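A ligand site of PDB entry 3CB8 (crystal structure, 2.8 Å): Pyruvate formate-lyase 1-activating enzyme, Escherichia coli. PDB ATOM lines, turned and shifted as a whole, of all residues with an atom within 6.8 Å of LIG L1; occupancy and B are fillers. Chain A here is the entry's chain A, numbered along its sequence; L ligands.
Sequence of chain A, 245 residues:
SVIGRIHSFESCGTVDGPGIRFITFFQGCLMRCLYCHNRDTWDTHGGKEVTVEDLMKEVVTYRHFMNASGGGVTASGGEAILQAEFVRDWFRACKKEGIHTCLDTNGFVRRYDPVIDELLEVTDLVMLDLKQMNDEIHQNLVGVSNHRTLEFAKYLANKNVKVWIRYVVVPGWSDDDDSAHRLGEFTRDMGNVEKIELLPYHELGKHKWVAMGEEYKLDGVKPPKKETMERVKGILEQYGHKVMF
An oxygen (O1) of LG2 L2 is bound to an iron atom (FE2) of LIG L1 (2.1 Å).
SG of Cys 29 binds FE4 of LIG L1, 2.2 Å away. S2 of LIG L1 lies close to N of Cys 33, 3.5 Å away. SG of Cys 33 binds FE1 of LIG L1, at 2.3 Å. An iron atom (FE3) of LIG L1 is bound by the side-chain sulfur (SG) of Cys 36 (2.3 Å). The indole nitrogen (NE1) of Trp 42 lies close to a sulfur (S2) of LIG L1. ND2 of Asn 106 lies close to S3 of LIG L1 (3.4 Å). The backbone carbonyl oxygen (O) of Gly 78 lies close to a nitrogen (N1) of LG2 L2. NZ of Lys 131 lies within hydrogen-bond range of O5 of LG2 L2, at 3.1 Å. The backbone carbonyl oxygen (O) of Tyr 35 is in hydrogen-bond range of a nitrogen (N4) of LG2 L2 (2.5 Å). OE2 of Glu 79 sits close to N1 of LG2 L2, 3.6 Å away. The backbone NH of His 37 sits at hydrogen-bond distance from a nitrogen (N3) of LG2 L2 (3.3 Å). A ring nitrogen (NE2) of His 37 sits at hydrogen-bond distance from an oxygen (O3) of LG2 L2 (3.3 Å). The side-chain carboxylate (OD1) of Asp 129 lies within hydrogen-bond range of an oxygen (O4) of LG2 L2 (2.8 Å).
SG of Cys 29 lies close to N of Met 31. The backbone carbonyl oxygen (O) of Cys 29 lies within hydrogen-bond range of the guanidinium group (NH2) of Arg 32, at 2.6 Å. SG of Cys 36 lies close to NE1 of Trp 42 (3.3 Å). The backbone NH of Asn 38 sits close to the side-chain sulfur of Cys 36 (3.4 Å). SG of Cys 36 sits close to N of Arg 39 (3.7 Å). The side-chain carboxylate (OE2) of Glu 79 lies within hydrogen-bond range of the side-chain amide nitrogen (ND2) of Asn 106 (3.0 Å). The side-chain amino group (NZ) of Lys 131 lies within hydrogen-bond range of the side-chain hydroxyl (OH) of Tyr 35 (3.0 Å). NZ of Lys 131 lies within salt-bridge range of OD2 of Asp 129.
The backbone carbonyl oxygen (O) of Met 31 lies close to a sulfur (S2) of LIG L1. The backbone carbonyl oxygen of Gly 77 lies close to a sulfur (S1) of LIG L1 (3.7 Å). Residues that only touch LIG L1: Thr 41, Gly 78 and Lys 131. Hydrophobic or aromatic side chains within 4 Å of LIG L1: Met 31 and Trp 42. The nearest printed residue that does not touch LIG L1 is Arg 32 (4.03 Å).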
ATOM      1  N   GLY A  28      20.672 -34.736  14.095  1.00  0.00           N
ATOM      2  CA  GLY A  28      20.771 -34.439  12.678  1.00  0.00           C
ATOM      3  C   GLY A  28      21.091 -33.008  12.295  1.00  0.00           C
ATOM      4  O   GLY A  28      20.585 -32.056  12.879  1.00  0.00           O
ATOM      5  N   CYS A  29      21.950 -32.882  11.295  1.00  0.00           N
ATOM      6  CA  CYS A  29      22.343 -31.581  10.785  1.00  0.00           C
ATOM      7  C   CYS A  29      22.856 -31.737   9.362  1.00  0.00           C
ATOM      8  O   CYS A  29      23.590 -32.666   9.046  1.00  0.00           O
ATOM      9  CB  CYS A  29      23.418 -30.959  11.661  1.00  0.00           C
ATOM     10  SG  CYS A  29      23.769 -29.253  11.176  1.00  0.00           S
ATOM     11  N   LEU A  30      22.470 -30.827   8.473  1.00  0.00           N
ATOM     12  CA  LEU A  30      22.943 -30.918   7.106  1.00  0.00           C
ATOM     13  C   LEU A  30      24.295 -30.200   6.933  1.00  0.00           C
ATOM     14  O   LEU A  30      25.049 -30.506   6.021  1.00  0.00           O
ATOM     15  CB  LEU A  30      21.898 -30.348   6.154  1.00  0.00           C
ATOM     16  CG  LEU A  30      20.512 -30.995   6.271  1.00  0.00           C
ATOM     17  CD1 LEU A  30      19.638 -30.499   5.136  1.00  0.00           C
ATOM     18  CD2 LEU A  30      20.611 -32.511   6.242  1.00  0.00           C
ATOM     19  N   MET A  31      24.614 -29.259   7.804  1.00  0.00           N
ATOM     20  CA  MET A  31      25.880 -28.571   7.656  1.00  0.00           C
ATOM     21  C   MET A  31      27.034 -29.399   8.189  1.00  0.00           C
ATOM     22  O   MET A  31      26.832 -30.443   8.806  1.00  0.00           O
ATOM     23  CB  MET A  31      25.823 -27.214   8.324  1.00  0.00           C
ATOM     24  CG  MET A  31      24.722 -26.334   7.791  1.00  0.00           C
ATOM     25  SD  MET A  31      24.988 -24.611   8.267  1.00  0.00           S
ATOM     26  CE  MET A  31      24.553 -23.748   6.756  1.00  0.00           C
ATOM     27  N   ARG A  32      28.254 -28.932   7.931  1.00  0.00           N
ATOM     28  CA  ARG A  32      29.462 -29.610   8.373  1.00  0.00           C
ATOM     29  C   ARG A  32      30.513 -28.613   8.837  1.00  0.00           C
ATOM     30  O   ARG A  32      31.656 -28.673   8.403  1.00  0.00           O
ATOM     31  CB  ARG A  32      30.072 -30.425   7.224  1.00  0.00           C
ATOM     32  CG  ARG A  32      29.148 -31.442   6.591  1.00  0.00           C
ATOM     33  CD  ARG A  32      28.634 -32.384   7.629  1.00  0.00           C
ATOM     34  NE  ARG A  32      27.867 -33.495   7.094  1.00  0.00           N
ATOM     35  CZ  ARG A  32      26.669 -33.855   7.547  1.00  0.00           C
ATOM     36  NH1 ARG A  32      26.045 -34.894   7.004  1.00  0.00           N
ATOM     37  NH2 ARG A  32      26.091 -33.164   8.523  1.00  0.00           N
ATOM     38  N   CYS A  33      30.123 -27.674   9.690  1.00  0.00           N
ATOM     39  CA  CYS A  33      31.054 -26.688  10.214  1.00  0.00           C
ATOM     40  C   CYS A  33      32.293 -27.425  10.694  1.00  0.00           C
ATOM     41  O   CYS A  33      32.207 -28.505  11.272  1.00  0.00           O
ATOM     42  CB  CYS A  33      30.409 -25.930  11.368  1.00  0.00           C
ATOM     43  SG  CYS A  33      28.764 -25.259  10.951  1.00  0.00           S
ATOM     44  N   LEU A  34      33.459 -26.865  10.443  1.00  0.00           N
ATOM     45  CA  LEU A  34      34.689 -27.518  10.859  1.00  0.00           C
ATOM     46  C   LEU A  34      34.898 -27.468  12.365  1.00  0.00           C
ATOM     47  O   LEU A  34      35.630 -28.304  12.903  1.00  0.00           O
ATOM     48  CB  LEU A  34      35.889 -26.886  10.150  1.00  0.00           C
ATOM     49  CG  LEU A  34      36.524 -27.536   8.908  1.00  0.00           C
ATOM     50  CD1 LEU A  34      35.527 -28.259   8.052  1.00  0.00           C
ATOM     51  CD2 LEU A  34      37.214 -26.437   8.132  1.00  0.00           C
ATOM     52  N   TYR A  35      34.280 -26.503  13.047  1.00  0.00           N
ATOM     53  CA  TYR A  35      34.456 -26.342  14.484  1.00  0.00           C
ATOM     54  C   TYR A  35      33.396 -26.985  15.353  1.00  0.00           C
ATOM     55  O   TYR A  35      33.496 -26.992  16.590  1.00  0.00           O
ATOM     56  CB  TYR A  35      34.566 -24.857  14.816  1.00  0.00           C
ATOM     57  CG  TYR A  35      33.401 -24.038  14.321  1.00  0.00           C
ATOM     58  CD1 TYR A  35      32.161 -24.126  14.952  1.00  0.00           C
ATOM     59  CD2 TYR A  35      33.529 -23.213  13.207  1.00  0.00           C
ATOM     60  CE1 TYR A  35      31.061 -23.410  14.485  1.00  0.00           C
ATOM     61  CE2 TYR A  35      32.433 -22.483  12.737  1.00  0.00           C
ATOM     62  CZ  TYR A  35      31.205 -22.593  13.384  1.00  0.00           C
ATOM     63  OH  TYR A  35      30.124 -21.890  12.916  1.00  0.00           O
ATOM     64  N   CYS A  36      32.372 -27.532  14.700  1.00  0.00           N
ATOM     65  CA  CYS A  36      31.267 -28.191  15.379  1.00  0.00           C
ATOM     66  C   CYS A  36      31.642 -29.000  16.603  1.00  0.00           C
ATOM     67  O   CYS A  36      32.377 -29.994  16.502  1.00  0.00           O
ATOM     68  CB  CYS A  36      30.539 -29.123  14.421  1.00  0.00           C
ATOM     69  SG  CYS A  36      29.034 -29.754  15.180  1.00  0.00           S
ATOM     70  N   HIS A  37      31.132 -28.619  17.768  1.00  0.00           N
ATOM     71  CA  HIS A  37      31.473 -29.382  18.957  1.00  0.00           C
ATOM     72  C   HIS A  37      30.489 -30.521  19.221  1.00  0.00           C
ATOM     73  O   HIS A  37      30.665 -31.289  20.162  1.00  0.00           O
ATOM     74  CB  HIS A  37      31.613 -28.472  20.177  1.00  0.00           C
ATOM     75  CG  HIS A  37      30.505 -27.483  20.349  1.00  0.00           C
ATOM     76  ND1 HIS A  37      30.662 -26.305  21.054  1.00  0.00           N
ATOM     77  CD2 HIS A  37      29.218 -27.513  19.929  1.00  0.00           C
ATOM     78  CE1 HIS A  37      29.517 -25.646  21.062  1.00  0.00           C
ATOM     79  NE2 HIS A  37      28.618 -26.355  20.389  1.00  0.00           N
ATOM     80  N   ASN A  38      29.465 -30.640  18.382  1.00  0.00           N
ATOM     81  CA  ASN A  38      28.509 -31.735  18.525  1.00  0.00           C
ATOM     82  C   ASN A  38      28.561 -32.541  17.250  1.00  0.00           C
ATOM     83  O   ASN A  38      27.536 -32.725  16.588  1.00  0.00           O
ATOM     84  CB  ASN A  38      27.063 -31.238  18.687  1.00  0.00           C
ATOM     85  CG  ASN A  38      26.912 -30.237  19.796  1.00  0.00           C
ATOM     86  OD1 ASN A  38      27.393 -30.444  20.915  1.00  0.00           O
ATOM     87  ND2 ASN A  38      26.227 -29.137  19.498  1.00  0.00           N
ATOM     88  N   ARG A  39      29.737 -33.013  16.866  1.00  0.00           N
ATOM     89  CA  ARG A  39      29.809 -33.747  15.624  1.00  0.00           C
ATOM     90  C   ARG A  39      28.912 -34.976  15.645  1.00  0.00           C
ATOM     91  O   ARG A  39      28.391 -35.388  14.608  1.00  0.00           O
ATOM     92  CB  ARG A  39      31.252 -34.146  15.289  1.00  0.00           C
ATOM     93  CG  ARG A  39      31.442 -34.375  13.787  1.00  0.00           C
ATOM     94  CD  ARG A  39      32.281 -35.577  13.528  1.00  0.00           C
ATOM     95  NE  ARG A  39      31.962 -36.218  12.249  1.00  0.00           N
ATOM     96  CZ  ARG A  39      30.771 -36.746  11.939  1.00  0.00           C
ATOM     97  NH1 ARG A  39      30.583 -37.315  10.755  1.00  0.00           N
ATOM     98  NH2 ARG A  39      29.774 -36.689  12.801  1.00  0.00           N
ATOM     99  N   THR A  41      26.187 -35.122  16.388  1.00  0.00           N
ATOM    100  CA  THR A  41      24.844 -34.605  16.253  1.00  0.00           C
ATOM    101  C   THR A  41      24.357 -34.623  14.798  1.00  0.00           C
ATOM    102  O   THR A  41      23.175 -34.498  14.533  1.00  0.00           O
ATOM    103  CB  THR A  41      24.828 -33.177  16.807  1.00  0.00           C
ATOM    104  OG1 THR A  41      23.992 -33.139  17.962  1.00  0.00           O
ATOM    105  CG2 THR A  41      24.358 -32.185  15.767  1.00  0.00           C
ATOM    106  N   TRP A  42      25.306 -34.801  13.891  1.00  0.00           N
ATOM    107  CA  TRP A  42      25.038 -34.797  12.464  1.00  0.00           C
ATOM    108  C   TRP A  42      24.119 -35.890  11.923  1.00  0.00           C
ATOM    109  O   TRP A  42      23.156 -35.604  11.214  1.00  0.00           O
ATOM    110  CB  TRP A  42      26.369 -34.878  11.728  1.00  0.00           C
ATOM    111  CG  TRP A  42      27.280 -33.720  11.993  1.00  0.00           C
ATOM    112  CD1 TRP A  42      27.055 -32.680  12.862  1.00  0.00           C
ATOM    113  CD2 TRP A  42      28.530 -33.447  11.359  1.00  0.00           C
ATOM    114  NE1 TRP A  42      28.088 -31.783  12.793  1.00  0.00           N
ATOM    115  CE2 TRP A  42      29.001 -32.227  11.874  1.00  0.00           C
ATOM    116  CE3 TRP A  42      29.297 -34.127  10.394  1.00  0.00           C
ATOM    117  CZ2 TRP A  42      30.217 -31.658  11.456  1.00  0.00           C
ATOM    118  CZ3 TRP A  42      30.500 -33.561   9.982  1.00  0.00           C
ATOM    119  CH2 TRP A  42      30.947 -32.337  10.515  1.00  0.00           C
ATOM    120  N   GLY A  77      20.844 -28.363  19.350  1.00  0.00           N
ATOM    121  CA  GLY A  77      21.424 -29.675  19.062  1.00  0.00           C
ATOM    122  C   GLY A  77      22.232 -29.676  17.787  1.00  0.00           C
ATOM    123  O   GLY A  77      23.388 -29.266  17.762  1.00  0.00           O
ATOM    124  N   GLY A  78      21.599 -30.216  16.750  1.00  0.00           N
ATOM    125  CA  GLY A  78      22.151 -30.244  15.421  1.00  0.00           C
ATOM    126  C   GLY A  78      21.292 -29.144  14.826  1.00  0.00           C
ATOM    127  O   GLY A  78      21.379 -28.005  15.286  1.00  0.00           O
ATOM    128  N   GLU A  79      20.453 -29.466  13.847  1.00  0.00           N
ATOM    129  CA  GLU A  79      19.576 -28.461  13.279  1.00  0.00           C
ATOM    130  C   GLU A  79      18.115 -28.751  13.572  1.00  0.00           C
ATOM    131  O   GLU A  79      17.473 -29.553  12.878  1.00  0.00           O
ATOM    132  CB  GLU A  79      19.778 -28.308  11.773  1.00  0.00           C
ATOM    133  CG  GLU A  79      18.940 -27.165  11.220  1.00  0.00           C
ATOM    134  CD  GLU A  79      18.999 -25.910  12.110  1.00  0.00           C
ATOM    135  OE1 GLU A  79      18.011 -25.138  12.137  1.00  0.00           O
ATOM    136  OE2 GLU A  79      20.031 -25.687  12.783  1.00  0.00           O
ATOM    137  N   THR A 105      19.158 -21.809  15.676  1.00  0.00           N
ATOM    138  CA  THR A 105      19.354 -22.394  14.354  1.00  0.00           C
ATOM    139  C   THR A 105      20.445 -21.813  13.427  1.00  0.00           C
ATOM    140  O   THR A 105      21.035 -20.777  13.696  1.00  0.00           O
ATOM    141  CB  THR A 105      17.982 -22.382  13.608  1.00  0.00           C
ATOM    142  OG1 THR A 105      18.137 -22.814  12.247  1.00  0.00           O
ATOM    143  CG2 THR A 105      17.401 -20.989  13.608  1.00  0.00           C
ATOM    144  N   ASN A 106      20.696 -22.534  12.335  1.00  0.00           N
ATOM    145  CA  ASN A 106      21.653 -22.121  11.320  1.00  0.00           C
ATOM    146  C   ASN A 106      20.875 -21.540  10.121  1.00  0.00           C
ATOM    147  O   ASN A 106      21.450 -21.081   9.130  1.00  0.00           O
ATOM    148  CB  ASN A 106      22.505 -23.318  10.866  1.00  0.00           C
ATOM    149  CG  ASN A 106      21.664 -24.465  10.346  1.00  0.00           C
ATOM    150  OD1 ASN A 106      20.668 -24.264   9.652  1.00  0.00           O
ATOM    151  ND2 ASN A 106      22.079 -25.683  10.655  1.00  0.00           N
ATOM    152  N   ASP A 129      22.429 -18.083  13.466  1.00  0.00           N
ATOM    153  CA  ASP A 129      23.857 -18.093  13.261  1.00  0.00           C
ATOM    154  C   ASP A 129      24.176 -17.632  11.864  1.00  0.00           C
ATOM    155  O   ASP A 129      23.548 -18.069  10.908  1.00  0.00           O
ATOM    156  CB  ASP A 129      24.413 -19.491  13.416  1.00  0.00           C
ATOM    157  CG  ASP A 129      25.193 -19.668  14.677  1.00  0.00           C
ATOM    158  OD1 ASP A 129      24.573 -19.616  15.771  1.00  0.00           O
ATOM    159  OD2 ASP A 129      26.429 -19.869  14.577  1.00  0.00           O
ATOM    160  N   LYS A 131      27.444 -17.702   9.925  1.00  0.00           N
ATOM    161  CA  LYS A 131      28.794 -18.211  10.044  1.00  0.00           C
ATOM    162  C   LYS A 131      29.859 -17.537   9.181  1.00  0.00           C
ATOM    163  O   LYS A 131      31.034 -17.552   9.538  1.00  0.00           O
ATOM    164  CB  LYS A 131      28.758 -19.736   9.810  1.00  0.00           C
ATOM    165  CG  LYS A 131      27.925 -20.426  10.886  1.00  0.00           C
ATOM    166  CD  LYS A 131      27.575 -21.872  10.587  1.00  0.00           C
ATOM    167  CE  LYS A 131      26.641 -22.449  11.665  1.00  0.00           C
ATOM    168  NZ  LYS A 131      27.255 -22.579  13.012  1.00  0.00           N
ATOM    169  N   VAL A 142      31.811 -24.244   6.295  1.00  0.00           N
ATOM    170  CA  VAL A 142      30.584 -24.977   6.598  1.00  0.00           C
ATOM    171  C   VAL A 142      30.261 -26.113   5.645  1.00  0.00           C
ATOM    172  O   VAL A 142      29.548 -27.030   6.002  1.00  0.00           O
ATOM    173  CB  VAL A 142      29.396 -24.006   6.592  1.00  0.00           C
ATOM    174  CG1 VAL A 142      28.140 -24.717   7.003  1.00  0.00           C
ATOM    175  CG2 VAL A 142      29.696 -22.839   7.494  1.00  0.00           C
HETATM  176 FE1  LIG L   1      27.376 -26.466  12.260  1.00  0.00          FE
HETATM  177 FE2  LIG L   1      25.495 -26.290  14.244  1.00  0.00          FE
HETATM  178 FE3  LIG L   1      27.480 -28.383  14.162  1.00  0.00          FE
HETATM  179 FE4  LIG L   1      25.402 -28.276  12.349  1.00  0.00          FE
HETATM  180  S1  LIG L   1      25.240 -28.558  14.629  1.00  0.00           S
HETATM  181  S2  LIG L   1      27.623 -28.725  11.909  1.00  0.00           S
HETATM  182  S3  LIG L   1      25.145 -26.034  11.977  1.00  0.00           S
HETATM  183  S4  LIG L   1      27.790 -26.134  14.496  1.00  0.00           S
HETATM  184  N1  LG2 L   2      23.333 -26.168  14.234  1.00  0.00           N
HETATM  185  C1  LG2 L   2      22.860 -24.908  14.838  1.00  0.00           C
HETATM  186  C2  LG2 L   2      23.963 -23.831  14.724  1.00  0.00           C
HETATM  187  O1  LG2 L   2      25.139 -24.222  14.562  1.00  0.00           O
HETATM  188  O2  LG2 L   2      23.587 -22.640  14.781  1.00  0.00           O
HETATM  189  C3  LG2 L   2      22.464 -25.169  16.304  1.00  0.00           C
HETATM  190  C4  LG2 L   2      23.462 -26.125  16.988  1.00  0.00           C
HETATM  191  S1  LG2 L   2      25.072 -25.330  17.286  1.00  0.00           S
HETATM  192  C5  LG2 L   2      26.318 -26.615  17.654  1.00  0.00           C
HETATM  193  C6  LG2 L   2      24.906 -24.181  18.706  1.00  0.00           C
HETATM  194  C7  LG2 L   2      25.975 -23.060  18.745  1.00  0.00           C
HETATM  195  O3  LG2 L   2      27.302 -23.636  18.987  1.00  0.00           O
HETATM  196  C8  LG2 L   2      26.073 -22.319  17.399  1.00  0.00           C
HETATM  197  O4  LG2 L   2      26.136 -20.912  17.673  1.00  0.00           O
HETATM  198  C9  LG2 L   2      27.391 -22.851  16.831  1.00  0.00           C
HETATM  199  O5  LG2 L   2      27.940 -21.907  15.925  1.00  0.00           O
HETATM  200  C10 LG2 L   2      28.212 -22.911  18.122  1.00  0.00           C
HETATM  201  N2  LG2 L   2      29.494 -23.696  17.987  1.00  0.00           N
HETATM  202  C11 LG2 L   2      29.621 -24.930  17.455  1.00  0.00           C
HETATM  203  N3  LG2 L   2      30.892 -25.338  17.553  1.00  0.00           N
HETATM  204  C12 LG2 L   2      31.582 -24.370  18.151  1.00  0.00           C
HETATM  205  C13 LG2 L   2      32.916 -24.223  18.520  1.00  0.00           C
HETATM  206  N4  LG2 L   2      33.799 -25.202  18.287  1.00  0.00           N
HETATM  207  N5  LG2 L   2      33.326 -23.079  19.139  1.00  0.00           N
HETATM  208  C14 LG2 L   2      32.452 -22.089  19.392  1.00  0.00           C
HETATM  209  N6  LG2 L   2      31.162 -22.206  19.043  1.00  0.00           N
HETATM  210  C15 LG2 L   2      30.703 -23.326  18.431  1.00  0.00           C
